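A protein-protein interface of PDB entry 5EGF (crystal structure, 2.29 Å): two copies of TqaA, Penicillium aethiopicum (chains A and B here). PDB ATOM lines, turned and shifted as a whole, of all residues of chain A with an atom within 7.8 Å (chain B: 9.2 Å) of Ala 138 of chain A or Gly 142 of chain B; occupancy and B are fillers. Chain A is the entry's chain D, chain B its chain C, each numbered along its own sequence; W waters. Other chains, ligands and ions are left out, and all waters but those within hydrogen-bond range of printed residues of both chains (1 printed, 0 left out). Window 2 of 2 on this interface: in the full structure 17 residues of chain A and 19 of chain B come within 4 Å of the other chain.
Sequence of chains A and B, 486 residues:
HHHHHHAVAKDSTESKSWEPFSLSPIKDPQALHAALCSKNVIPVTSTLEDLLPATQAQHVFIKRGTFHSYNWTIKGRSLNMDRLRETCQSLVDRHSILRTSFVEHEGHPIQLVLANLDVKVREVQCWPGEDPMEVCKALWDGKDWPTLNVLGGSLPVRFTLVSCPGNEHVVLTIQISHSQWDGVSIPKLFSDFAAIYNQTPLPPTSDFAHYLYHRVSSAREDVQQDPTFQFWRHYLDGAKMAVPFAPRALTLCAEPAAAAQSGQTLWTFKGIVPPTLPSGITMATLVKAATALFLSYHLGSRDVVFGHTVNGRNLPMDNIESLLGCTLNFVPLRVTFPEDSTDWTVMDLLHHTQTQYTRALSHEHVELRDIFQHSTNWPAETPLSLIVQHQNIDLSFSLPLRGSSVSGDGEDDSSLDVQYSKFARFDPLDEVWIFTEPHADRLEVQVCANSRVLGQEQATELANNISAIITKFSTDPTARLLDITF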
ATOM      1  N   ARG A 122      19.611  31.861 -11.658  1.00  0.00           N
ATOM      2  CA  ARG A 122      18.286  31.732 -12.253  1.00  0.00           C
ATOM      3  C   ARG A 122      17.328  32.486 -11.327  1.00  0.00           C
ATOM      4  O   ARG A 122      17.319  32.259 -10.106  1.00  0.00           O
ATOM      5  CB  ARG A 122      17.883  30.268 -12.419  1.00  0.00           C
ATOM      6  CG  ARG A 122      16.427  30.058 -12.810  1.00  0.00           C
ATOM      7  CD  ARG A 122      16.139  28.579 -13.052  1.00  0.00           C
ATOM      8  NE  ARG A 122      16.177  27.767 -11.830  1.00  0.00           N
ATOM      9  CZ  ARG A 122      16.015  26.445 -11.804  1.00  0.00           C
ATOM     10  NH1 ARG A 122      15.813  25.784 -12.933  1.00  0.00           N
ATOM     11  NH2 ARG A 122      16.056  25.787 -10.651  1.00  0.00           N
ATOM     12  N   GLU A 130       1.715  33.512  -4.574  1.00  0.00           N
ATOM     13  CA  GLU A 130       2.431  32.312  -4.997  1.00  0.00           C
ATOM     14  C   GLU A 130       3.658  32.018  -4.121  1.00  0.00           C
ATOM     15  O   GLU A 130       4.512  32.873  -3.957  1.00  0.00           O
ATOM     16  CB  GLU A 130       2.864  32.507  -6.455  1.00  0.00           C
ATOM     17  CG  GLU A 130       3.662  31.372  -7.089  1.00  0.00           C
ATOM     18  CD  GLU A 130       3.992  31.661  -8.558  1.00  0.00           C
ATOM     19  OE1 GLU A 130       4.306  32.834  -8.876  1.00  0.00           O
ATOM     20  OE2 GLU A 130       3.919  30.729  -9.400  1.00  0.00           O
ATOM     21  N   ASP A 131       3.743  30.804  -3.582  1.00  0.00           N
ATOM     22  CA  ASP A 131       4.831  30.402  -2.684  1.00  0.00           C
ATOM     23  C   ASP A 131       6.140  30.074  -3.432  1.00  0.00           C
ATOM     24  O   ASP A 131       6.195  29.140  -4.228  1.00  0.00           O
ATOM     25  CB  ASP A 131       4.381  29.201  -1.830  1.00  0.00           C
ATOM     26  CG  ASP A 131       5.461  28.710  -0.869  1.00  0.00           C
ATOM     27  OD1 ASP A 131       6.213  29.545  -0.319  1.00  0.00           O
ATOM     28  OD2 ASP A 131       5.557  27.478  -0.650  1.00  0.00           O
ATOM     29  N   PRO A 132       7.212  30.842  -3.167  1.00  0.00           N
ATOM     30  CA  PRO A 132       8.478  30.566  -3.862  1.00  0.00           C
ATOM     31  C   PRO A 132       8.944  29.119  -3.682  1.00  0.00           C
ATOM     32  O   PRO A 132       9.342  28.514  -4.677  1.00  0.00           O
ATOM     33  CB  PRO A 132       9.462  31.534  -3.204  1.00  0.00           C
ATOM     34  CG  PRO A 132       8.617  32.634  -2.669  1.00  0.00           C
ATOM     35  CD  PRO A 132       7.322  31.994  -2.251  1.00  0.00           C
ATOM     36  N   MET A 133       8.891  28.569  -2.464  1.00  0.00           N
ATOM     37  CA  MET A 133       9.310  27.175  -2.264  1.00  0.00           C
ATOM     38  C   MET A 133       8.560  26.225  -3.194  1.00  0.00           C
ATOM     39  O   MET A 133       9.180  25.339  -3.776  1.00  0.00           O
ATOM     40  CB  MET A 133       9.180  26.737  -0.806  1.00  0.00           C
ATOM     41  CG  MET A 133       9.795  25.386  -0.537  1.00  0.00           C
ATOM     42  SD  MET A 133      11.777  25.323  -0.837  1.00  0.00           S
ATOM     43  CE  MET A 133      12.297  26.414   0.615  1.00  0.00           C
ATOM     44  N   GLU A 134       7.245  26.427  -3.350  1.00  0.00           N
ATOM     45  CA  GLU A 134       6.437  25.626  -4.276  1.00  0.00           C
ATOM     46  C   GLU A 134       6.942  25.787  -5.694  1.00  0.00           C
ATOM     47  O   GLU A 134       6.989  24.831  -6.469  1.00  0.00           O
ATOM     48  CB  GLU A 134       4.948  26.009  -4.221  1.00  0.00           C
ATOM     49  CG  GLU A 134       4.265  25.680  -2.894  1.00  0.00           C
ATOM     50  CD  GLU A 134       2.795  26.088  -2.856  1.00  0.00           C
ATOM     51  OE1 GLU A 134       2.194  26.292  -3.941  1.00  0.00           O
ATOM     52  OE2 GLU A 134       2.239  26.196  -1.734  1.00  0.00           O
ATOM     53  N   VAL A 135       7.308  27.006  -6.056  1.00  0.00           N
ATOM     54  CA  VAL A 135       7.945  27.208  -7.357  1.00  0.00           C
ATOM     55  C   VAL A 135       9.276  26.448  -7.480  1.00  0.00           C
ATOM     56  O   VAL A 135       9.555  25.818  -8.505  1.00  0.00           O
ATOM     57  CB  VAL A 135       8.154  28.694  -7.672  1.00  0.00           C
ATOM     58  CG1 VAL A 135       9.191  28.840  -8.779  1.00  0.00           C
ATOM     59  CG2 VAL A 135       6.828  29.343  -8.075  1.00  0.00           C
ATOM     60  N   CYS A 136      10.089  26.484  -6.429  1.00  0.00           N
ATOM     61  CA  CYS A 136      11.341  25.745  -6.465  1.00  0.00           C
ATOM     62  C   CYS A 136      11.089  24.271  -6.709  1.00  0.00           C
ATOM     63  O   CYS A 136      11.745  23.671  -7.563  1.00  0.00           O
ATOM     64  CB  CYS A 136      12.138  25.930  -5.173  1.00  0.00           C
ATOM     65  SG  CYS A 136      12.742  27.609  -5.003  1.00  0.00           S
ATOM     66  N   LYS A 137      10.132  23.717  -5.957  1.00  0.00           N
ATOM     67  CA  LYS A 137       9.798  22.296  -5.994  1.00  0.00           C
ATOM     68  C   LYS A 137       9.345  21.924  -7.393  1.00  0.00           C
ATOM     69  O   LYS A 137       9.691  20.868  -7.907  1.00  0.00           O
ATOM     70  CB  LYS A 137       8.708  21.984  -4.971  1.00  0.00           C
ATOM     71  CG  LYS A 137       8.627  20.522  -4.576  1.00  0.00           C
ATOM     72  CD  LYS A 137      10.024  19.853  -4.592  1.00  0.00           C
ATOM     73  CE  LYS A 137      10.044  18.481  -3.877  1.00  0.00           C
ATOM     74  NZ  LYS A 137       8.964  17.515  -4.311  1.00  0.00           N
ATOM     75  N   ALA A 138       8.609  22.825  -8.033  1.00  0.00           N
ATOM     76  CA  ALA A 138       8.129  22.582  -9.388  1.00  0.00           C
ATOM     77  C   ALA A 138       9.273  22.534 -10.406  1.00  0.00           C
ATOM     78  O   ALA A 138       9.205  21.825 -11.400  1.00  0.00           O
ATOM     79  CB  ALA A 138       7.085  23.640  -9.799  1.00  0.00           C
ATOM     80  N   LEU A 139      10.315  23.320 -10.186  1.00  0.00           N
ATOM     81  CA  LEU A 139      11.405  23.335 -11.156  1.00  0.00           C
ATOM     82  C   LEU A 139      12.265  22.108 -10.894  1.00  0.00           C
ATOM     83  O   LEU A 139      12.739  21.473 -11.825  1.00  0.00           O
ATOM     84  CB  LEU A 139      12.195  24.648 -11.090  1.00  0.00           C
ATOM     85  CG  LEU A 139      11.383  25.892 -11.461  1.00  0.00           C
ATOM     86  CD1 LEU A 139      12.119  27.159 -11.076  1.00  0.00           C
ATOM     87  CD2 LEU A 139      11.063  25.883 -12.943  1.00  0.00           C
ATOM     88  N   TRP A 140      12.406  21.761  -9.621  1.00  0.00           N
ATOM     89  CA  TRP A 140      13.152  20.582  -9.218  1.00  0.00           C
ATOM     90  C   TRP A 140      12.567  19.319  -9.825  1.00  0.00           C
ATOM     91  O   TRP A 140      13.240  18.629 -10.582  1.00  0.00           O
ATOM     92  CB  TRP A 140      13.118  20.459  -7.714  1.00  0.00           C
ATOM     93  CG  TRP A 140      13.826  19.260  -7.149  1.00  0.00           C
ATOM     94  CD1 TRP A 140      13.243  18.147  -6.603  1.00  0.00           C
ATOM     95  CD2 TRP A 140      15.249  19.068  -7.028  1.00  0.00           C
ATOM     96  NE1 TRP A 140      14.214  17.280  -6.149  1.00  0.00           N
ATOM     97  CE2 TRP A 140      15.451  17.817  -6.401  1.00  0.00           C
ATOM     98  CE3 TRP A 140      16.362  19.822  -7.393  1.00  0.00           C
ATOM     99  CZ2 TRP A 140      16.724  17.313  -6.124  1.00  0.00           C
ATOM    100  CZ3 TRP A 140      17.638  19.318  -7.115  1.00  0.00           C
ATOM    101  CH2 TRP A 140      17.808  18.077  -6.490  1.00  0.00           C
ATOM    102  N   ASP A 141      11.321  19.004  -9.473  1.00  0.00           N
ATOM    103  CA  ASP A 141      10.661  17.808  -9.993  1.00  0.00           C
ATOM    104  C   ASP A 141      10.383  17.889 -11.500  1.00  0.00           C
ATOM    105  O   ASP A 141      10.286  16.859 -12.170  1.00  0.00           O
ATOM    106  CB  ASP A 141       9.341  17.566  -9.263  1.00  0.00           C
ATOM    107  CG  ASP A 141       9.531  17.187  -7.812  1.00  0.00           C
ATOM    108  OD1 ASP A 141      10.592  16.624  -7.475  1.00  0.00           O
ATOM    109  OD2 ASP A 141       8.607  17.449  -7.003  1.00  0.00           O
ATOM    110  N   GLY A 142      10.243  19.109 -12.025  1.00  0.00           N
ATOM    111  CA  GLY A 142       9.883  19.306 -13.420  1.00  0.00           C
ATOM    112  C   GLY A 142      11.013  19.125 -14.425  1.00  0.00           C
ATOM    113  O   GLY A 142      10.826  18.524 -15.482  1.00  0.00           O
ATOM    114  N   LYS A 143      12.192  19.648 -14.120  1.00  0.00           N
ATOM    115  CA  LYS A 143      13.303  19.543 -15.056  1.00  0.00           C
ATOM    116  C   LYS A 143      14.647  19.278 -14.382  1.00  0.00           C
ATOM    117  O   LYS A 143      15.372  18.354 -14.772  1.00  0.00           O
ATOM    118  CB  LYS A 143      13.387  20.790 -15.958  1.00  0.00           C
ATOM    119  CG  LYS A 143      13.293  22.125 -15.216  1.00  0.00           C
ATOM    120  CD  LYS A 143      13.096  23.291 -16.185  1.00  0.00           C
ATOM    121  CE  LYS A 143      14.210  23.338 -17.226  1.00  0.00           C
ATOM    122  NZ  LYS A 143      15.556  23.506 -16.602  1.00  0.00           N
ATOM    123  N   ASP A 144      14.966  20.073 -13.366  1.00  0.00           N
ATOM    124  CA  ASP A 144      16.292  20.032 -12.731  1.00  0.00           C
ATOM    125  C   ASP A 144      16.895  18.649 -12.470  1.00  0.00           C
ATOM    126  O   ASP A 144      18.020  18.379 -12.910  1.00  0.00           O
ATOM    127  CB  ASP A 144      16.324  20.883 -11.462  1.00  0.00           C
ATOM    128  CG  ASP A 144      15.984  22.316 -11.740  1.00  0.00           C
ATOM    129  OD1 ASP A 144      15.920  22.682 -12.939  1.00  0.00           O
ATOM    130  OD2 ASP A 144      15.764  23.072 -10.769  1.00  0.00           O
ATOM    131  N   PRO A 146      15.214  15.432 -13.189  1.00  0.00           N
ATOM    132  CA  PRO A 146      14.984  14.459 -14.271  1.00  0.00           C
ATOM    133  C   PRO A 146      15.954  14.598 -15.452  1.00  0.00           C
ATOM    134  O   PRO A 146      16.207  13.617 -16.135  1.00  0.00           O
ATOM    135  CB  PRO A 146      13.553  14.780 -14.744  1.00  0.00           C
ATOM    136  CG  PRO A 146      12.891  15.420 -13.571  1.00  0.00           C
ATOM    137  CD  PRO A 146      13.986  16.184 -12.844  1.00  0.00           C
ATOM    138  N   PHE A 423      16.217  19.585  -1.107  1.00  0.00           N
ATOM    139  CA  PHE A 423      15.736  18.555  -2.014  1.00  0.00           C
ATOM    140  C   PHE A 423      16.931  17.632  -2.232  1.00  0.00           C
ATOM    141  O   PHE A 423      18.068  18.125  -2.353  1.00  0.00           O
ATOM    142  CB  PHE A 423      15.342  19.147  -3.368  1.00  0.00           C
ATOM    143  CG  PHE A 423      14.253  20.192  -3.311  1.00  0.00           C
ATOM    144  CD1 PHE A 423      13.191  20.088  -2.408  1.00  0.00           C
ATOM    145  CD2 PHE A 423      14.279  21.278  -4.182  1.00  0.00           C
ATOM    146  CE1 PHE A 423      12.179  21.058  -2.378  1.00  0.00           C
ATOM    147  CE2 PHE A 423      13.280  22.234  -4.151  1.00  0.00           C
ATOM    148  CZ  PHE A 423      12.232  22.120  -3.251  1.00  0.00           C
ATOM    149  N   ARG B 122       4.493  37.198 -13.827  1.00  0.00           N
ATOM    150  CA  ARG B 122       5.446  36.279 -13.217  1.00  0.00           C
ATOM    151  C   ARG B 122       6.612  36.129 -14.179  1.00  0.00           C
ATOM    152  O   ARG B 122       6.410  35.800 -15.354  1.00  0.00           O
ATOM    153  CB  ARG B 122       4.812  34.923 -12.972  1.00  0.00           C
ATOM    154  CG  ARG B 122       5.828  33.815 -12.749  1.00  0.00           C
ATOM    155  CD  ARG B 122       5.150  32.525 -12.330  1.00  0.00           C
ATOM    156  NE  ARG B 122       4.595  31.793 -13.470  1.00  0.00           N
ATOM    157  CZ  ARG B 122       3.986  30.611 -13.379  1.00  0.00           C
ATOM    158  NH1 ARG B 122       3.839  30.024 -12.200  1.00  0.00           N
ATOM    159  NH2 ARG B 122       3.526  30.014 -14.472  1.00  0.00           N
ATOM    160  N   GLU B 130      19.465  26.996 -20.513  1.00  0.00           N
ATOM    161  CA  GLU B 130      18.173  26.481 -20.068  1.00  0.00           C
ATOM    162  C   GLU B 130      17.062  26.908 -21.033  1.00  0.00           C
ATOM    163  O   GLU B 130      16.897  28.090 -21.294  1.00  0.00           O
ATOM    164  CB  GLU B 130      17.887  26.978 -18.641  1.00  0.00           C
ATOM    165  CG  GLU B 130      16.637  26.406 -17.977  1.00  0.00           C
ATOM    166  CD  GLU B 130      16.486  26.846 -16.530  1.00  0.00           C
ATOM    167  OE1 GLU B 130      16.677  28.053 -16.238  1.00  0.00           O
ATOM    168  OE2 GLU B 130      16.175  25.986 -15.676  1.00  0.00           O
ATOM    169  N   GLU B 134      10.742  24.609 -21.562  1.00  0.00           N
ATOM    170  CA  GLU B 134      10.851  23.560 -20.566  1.00  0.00           C
ATOM    171  C   GLU B 134      10.592  24.118 -19.185  1.00  0.00           C
ATOM    172  O   GLU B 134      10.056  23.417 -18.329  1.00  0.00           O
ATOM    173  CB  GLU B 134      12.232  22.903 -20.597  1.00  0.00           C
ATOM    174  CG  GLU B 134      12.561  22.190 -21.897  1.00  0.00           C
ATOM    175  CD  GLU B 134      13.998  21.674 -21.920  1.00  0.00           C
ATOM    176  OE1 GLU B 134      14.597  21.502 -20.821  1.00  0.00           O
ATOM    177  OE2 GLU B 134      14.524  21.441 -23.040  1.00  0.00           O
ATOM    178  N   VAL B 135      11.006  25.365 -18.957  1.00  0.00           N
ATOM    179  CA  VAL B 135      10.704  26.026 -17.702  1.00  0.00           C
ATOM    180  C   VAL B 135       9.183  26.230 -17.553  1.00  0.00           C
ATOM    181  O   VAL B 135       8.606  25.957 -16.492  1.00  0.00           O
ATOM    182  CB  VAL B 135      11.415  27.378 -17.587  1.00  0.00           C
ATOM    183  CG1 VAL B 135      10.945  28.090 -16.349  1.00  0.00           C
ATOM    184  CG2 VAL B 135      12.951  27.195 -17.540  1.00  0.00           C
ATOM    185  N   CYS B 136       8.541  26.705 -18.618  1.00  0.00           N
ATOM    186  CA  CYS B 136       7.112  26.960 -18.578  1.00  0.00           C
ATOM    187  C   CYS B 136       6.403  25.646 -18.348  1.00  0.00           C
ATOM    188  O   CYS B 136       5.585  25.523 -17.433  1.00  0.00           O
ATOM    189  CB  CYS B 136       6.619  27.601 -19.888  1.00  0.00           C
ATOM    190  SG  CYS B 136       7.193  29.306 -20.159  1.00  0.00           S
ATOM    191  N   LYS B 137       6.739  24.662 -19.177  1.00  0.00           N
ATOM    192  CA  LYS B 137       6.169  23.334 -19.057  1.00  0.00           C
ATOM    193  C   LYS B 137       6.316  22.762 -17.636  1.00  0.00           C
ATOM    194  O   LYS B 137       5.382  22.158 -17.102  1.00  0.00           O
ATOM    195  CB  LYS B 137       6.790  22.407 -20.103  1.00  0.00           C
ATOM    196  CG  LYS B 137       6.130  21.041 -20.230  1.00  0.00           C
ATOM    197  CD  LYS B 137       4.652  21.152 -20.639  1.00  0.00           C
ATOM    198  CE  LYS B 137       4.136  19.849 -21.268  1.00  0.00           C
ATOM    199  NZ  LYS B 137       3.865  18.782 -20.269  1.00  0.00           N
ATOM    200  N   ALA B 138       7.471  22.971 -17.008  1.00  0.00           N
ATOM    201  CA  ALA B 138       7.662  22.503 -15.636  1.00  0.00           C
ATOM    202  C   ALA B 138       6.753  23.213 -14.644  1.00  0.00           C
ATOM    203  O   ALA B 138       6.265  22.602 -13.697  1.00  0.00           O
ATOM    204  CB  ALA B 138       9.128  22.643 -15.203  1.00  0.00           C
ATOM    205  N   LEU B 139       6.543  24.509 -14.846  1.00  0.00           N
ATOM    206  CA  LEU B 139       5.655  25.269 -13.977  1.00  0.00           C
ATOM    207  C   LEU B 139       4.228  24.763 -14.170  1.00  0.00           C
ATOM    208  O   LEU B 139       3.502  24.564 -13.198  1.00  0.00           O
ATOM    209  CB  LEU B 139       5.752  26.770 -14.273  1.00  0.00           C
ATOM    210  CG  LEU B 139       7.129  27.398 -14.022  1.00  0.00           C
ATOM    211  CD1 LEU B 139       7.130  28.863 -14.439  1.00  0.00           C
ATOM    212  CD2 LEU B 139       7.586  27.247 -12.563  1.00  0.00           C
ATOM    213  N   TRP B 140       3.856  24.533 -15.428  1.00  0.00           N
ATOM    214  CA  TRP B 140       2.529  24.038 -15.785  1.00  0.00           C
ATOM    215  C   TRP B 140       2.227  22.703 -15.091  1.00  0.00           C
ATOM    216  O   TRP B 140       1.239  22.587 -14.354  1.00  0.00           O
ATOM    217  CB  TRP B 140       2.424  23.921 -17.310  1.00  0.00           C
ATOM    218  CG  TRP B 140       1.085  23.475 -17.844  1.00  0.00           C
ATOM    219  CD1 TRP B 140       0.765  22.226 -18.300  1.00  0.00           C
ATOM    220  CD2 TRP B 140      -0.102  24.274 -18.005  1.00  0.00           C
ATOM    221  NE1 TRP B 140      -0.540  22.194 -18.718  1.00  0.00           N
ATOM    222  CE2 TRP B 140      -1.100  23.428 -18.547  1.00  0.00           C
ATOM    223  CE3 TRP B 140      -0.424  25.608 -17.729  1.00  0.00           C
ATOM    224  CZ2 TRP B 140      -2.409  23.885 -18.825  1.00  0.00           C
ATOM    225  CZ3 TRP B 140      -1.743  26.060 -18.012  1.00  0.00           C
ATOM    226  CH2 TRP B 140      -2.704  25.193 -18.557  1.00  0.00           C
ATOM    227  N   ASP B 141       3.081  21.706 -15.297  1.00  0.00           N
ATOM    228  CA  ASP B 141       2.850  20.383 -14.704  1.00  0.00           C
ATOM    229  C   ASP B 141       3.166  20.339 -13.224  1.00  0.00           C
ATOM    230  O   ASP B 141       2.547  19.581 -12.470  1.00  0.00           O
ATOM    231  CB  ASP B 141       3.651  19.307 -15.437  1.00  0.00           C
ATOM    232  CG  ASP B 141       3.207  19.146 -16.867  1.00  0.00           C
ATOM    233  OD1 ASP B 141       1.990  19.256 -17.115  1.00  0.00           O
ATOM    234  OD2 ASP B 141       4.064  18.944 -17.752  1.00  0.00           O
ATOM    235  N   GLY B 142       4.114  21.169 -12.808  1.00  0.00           N
ATOM    236  CA  GLY B 142       4.575  21.167 -11.435  1.00  0.00           C
ATOM    237  C   GLY B 142       3.648  21.848 -10.456  1.00  0.00           C
ATOM    238  O   GLY B 142       3.752  21.611  -9.252  1.00  0.00           O
ATOM    239  N   LYS B 143       2.742  22.692 -10.947  1.00  0.00           N
ATOM    240  CA  LYS B 143       1.897  23.457 -10.028  1.00  0.00           C
ATOM    241  C   LYS B 143       0.683  24.173 -10.631  1.00  0.00           C
ATOM    242  O   LYS B 143      -0.394  24.160 -10.037  1.00  0.00           O
ATOM    243  CB  LYS B 143       2.742  24.464  -9.228  1.00  0.00           C
ATOM    244  CG  LYS B 143       3.194  25.687 -10.010  1.00  0.00           C
ATOM    245  CD  LYS B 143       4.022  26.645  -9.139  1.00  0.00           C
ATOM    246  CE  LYS B 143       3.150  27.470  -8.211  1.00  0.00           C
ATOM    247  NZ  LYS B 143       2.215  28.317  -9.003  1.00  0.00           N
ATOM    248  N   ASP B 144       0.852  24.810 -11.788  1.00  0.00           N
ATOM    249  CA  ASP B 144      -0.213  25.665 -12.352  1.00  0.00           C
ATOM    250  C   ASP B 144      -1.567  24.960 -12.529  1.00  0.00           C
ATOM    251  O   ASP B 144      -2.548  25.388 -11.944  1.00  0.00           O
ATOM    252  CB  ASP B 144       0.224  26.383 -13.642  1.00  0.00           C
ATOM    253  CG  ASP B 144       1.442  27.317 -13.436  1.00  0.00           C
ATOM    254  OD1 ASP B 144       1.824  27.641 -12.280  1.00  0.00           O
ATOM    255  OD2 ASP B 144       2.034  27.726 -14.460  1.00  0.00           O
ATOM    256  N   TRP B 145      -1.641  23.869 -13.289  1.00  0.00           N
ATOM    257  CA  TRP B 145      -2.934  23.162 -13.368  1.00  0.00           C
ATOM    258  C   TRP B 145      -3.292  22.238 -12.179  1.00  0.00           C
ATOM    259  O   TRP B 145      -4.425  22.271 -11.698  1.00  0.00           O
ATOM    260  CB  TRP B 145      -3.168  22.489 -14.723  1.00  0.00           C
ATOM    261  CG  TRP B 145      -2.270  21.377 -15.051  1.00  0.00           C
ATOM    262  CD1 TRP B 145      -1.104  21.452 -15.754  1.00  0.00           C
ATOM    263  CD2 TRP B 145      -2.460  19.989 -14.732  1.00  0.00           C
ATOM    264  NE1 TRP B 145      -0.546  20.204 -15.880  1.00  0.00           N
ATOM    265  CE2 TRP B 145      -1.355  19.286 -15.263  1.00  0.00           C
ATOM    266  CE3 TRP B 145      -3.450  19.272 -14.042  1.00  0.00           C
ATOM    267  CZ2 TRP B 145      -1.211  17.896 -15.134  1.00  0.00           C
ATOM    268  CZ3 TRP B 145      -3.306  17.891 -13.907  1.00  0.00           C
ATOM    269  CH2 TRP B 145      -2.190  17.219 -14.453  1.00  0.00           C
ATOM    270  N   PRO B 146      -2.321  21.448 -11.677  1.00  0.00           N
ATOM    271  CA  PRO B 146      -2.568  20.515 -10.567  1.00  0.00           C
ATOM    272  C   PRO B 146      -3.130  21.193  -9.322  1.00  0.00           C
ATOM    273  O   PRO B 146      -3.610  20.512  -8.420  1.00  0.00           O
ATOM    274  CB  PRO B 146      -1.167  19.941 -10.271  1.00  0.00           C
ATOM    275  CG  PRO B 146      -0.427  20.088 -11.548  1.00  0.00           C
ATOM    276  CD  PRO B 146      -0.930  21.359 -12.165  1.00  0.00           C
ATOM    277  N   THR B 147      -3.040  22.515  -9.257  1.00  0.00           N
ATOM    278  CA  THR B 147      -3.535  23.243  -8.100  1.00  0.00           C
ATOM    279  C   THR B 147      -4.602  24.239  -8.537  1.00  0.00           C
ATOM    280  O   THR B 147      -5.090  25.025  -7.724  1.00  0.00           O
ATOM    281  CB  THR B 147      -2.409  24.015  -7.364  1.00  0.00           C
ATOM    282  OG1 THR B 147      -2.007  25.148  -8.150  1.00  0.00           O
ATOM    283  CG2 THR B 147      -1.215  23.105  -7.076  1.00  0.00           C
ATOM    284  N   LEU B 148      -4.951  24.223  -9.820  1.00  0.00           N
ATOM    285  CA  LEU B 148      -6.004  25.104 -10.302  1.00  0.00           C
ATOM    286  C   LEU B 148      -7.282  24.928  -9.480  1.00  0.00           C
ATOM    287  O   LEU B 148      -7.747  23.809  -9.285  1.00  0.00           O
ATOM    288  CB  LEU B 148      -6.312  24.828 -11.768  1.00  0.00           C
ATOM    289  CG  LEU B 148      -7.530  25.585 -12.280  1.00  0.00           C
ATOM    290  CD1 LEU B 148      -7.150  27.019 -12.663  1.00  0.00           C
ATOM    291  CD2 LEU B 148      -8.141  24.836 -13.448  1.00  0.00           C
HETATM  292  O   HOH W   1       9.215  20.072 -17.680  1.00  0.00           O
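NZ of Lys 143 of chain B is in salt-bridge range of OD1 of Asp 144 of chain B (3.4 Å). The backbone NH (N) of Asp 144 of chain A is in hydrogen-bond range of the backbone carbonyl oxygen (O) of Leu 139 of chain A. The side-chain carboxylate of Asp 144 of chain B is in salt-bridge range of the guanidinium group of Arg 122 of chain B. O of Leu 139 of chain B is in hydrogen-bond range of N of Asp 144 of chain B. The side-chain amino group (NZ) of Lys 143 of chain A lies within salt-bridge range of the side-chain carboxylate (OD1) of Asp 144 of chain A, 3.8 Å away.
Ala 138 of chain B touches Ala 138 of chain A. Gly 142 of chain B touches Ala 138 of chain A. Leu 139 of chain A touches Leu 139 of chain B (CD2 to CD2, 3.8 Å). CA of Gly 142 of chain A touches CB of Ala 138 of chain B, at 3.9 Å. Lys 143 of chain A touches Glu 134 of chain B (CD to O, 3.7 Å). Lys 143 of chain A touches Val 135 of chain B.
Ala 138 of chain A touches just these residues of chain B: Ala 138 and Gly 142. Gly 142 of chain B touches just one residue of chain A: Ala 138 (3.9 Å). Of the printed residues of chain A, Leu 139 of chain B touches Leu 139. Printed residues of chain A within 4 Å of Lys 143 of chain B: Glu 130 (3.0 Å). Asp 141 of chain A touches none of the printed residues of chain B. Lys 137 of chain B touches none of the printed residues of chain A. The nearest printed residue of chain A that does not touch Ala 138 of chain B is Lys 143 of chain A (4.1 Å).
The side-chain carboxylate of Glu 130 of chain B is in salt-bridge range of the side-chain amino group of Lys 143 of chain A. The side-chain carboxylate (OE2) of Glu 130 of chain B lies within salt-bridge range of the guanidinium group (NH1) of Arg 122 of chain A (2.8 Å). The guanidinium group (NH1) of Arg 122 of chain B is in salt-bridge range of the side-chain carboxylate (OE2) of Glu 130 of chain A. NZ of Lys 143 of chain B lies within salt-bridge range of OE2 of Glu 130 of chain A (3.0 Å).
Water W1 bridges O of Gly 142 of chain A (3.1 Å) and N of Ala 138 of chain B (3.4 Å).
Ala 138 of chain B touches its own counterpart, Ala 138 of chain A. Ala 138 of chain A touches Gly 142 of chain B, and with the chains exchanged Gly 142 of chain A touches Ala 138 of chain B. Leu 139 of chain A touches its own counterpart, Leu 139 of chain B. Lys 143 of chain A touches Glu 134 of chain B, but with the chains exchanged Glu 134 of chain A does not touch Lys 143 of chain B (4.4 Å). 14 positions are printed for both chains. Of the 10 pairs that touch across the chains among the printed residues, 8 have their exchanged pair printed and touching as well.
Of the 18 printed residues of chain A, 6 touch a printed residue of chain B. Hydrophobic or aromatic side chains of chain A within 4 Å of the printed part of chain B: Ala 138 and Leu 139. Of the 17 printed residues of chain B, 8 touch a printed residue of chain A. Printed residues of chain B that touch a printed residue of chain A: Arg 122, Glu 130, Glu 134, Val 135, Ala 138, Leu 139, Gly 142 and Lys 143. Among the printed residues, Asp or Glu carboxylates within 4 Å of a Lys or Arg side-chain nitrogen of the other chain: Arg 122 of chain A with Glu 130 of chain B (2.8 Å), Glu 130 of chain A with Arg 122 of chain B (2.9 Å), Glu 130 of chain A with Lys 143 of chain B (3.0 Å) and Lys 143 of chain A with Glu 130 of chain B (2.7 Å).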
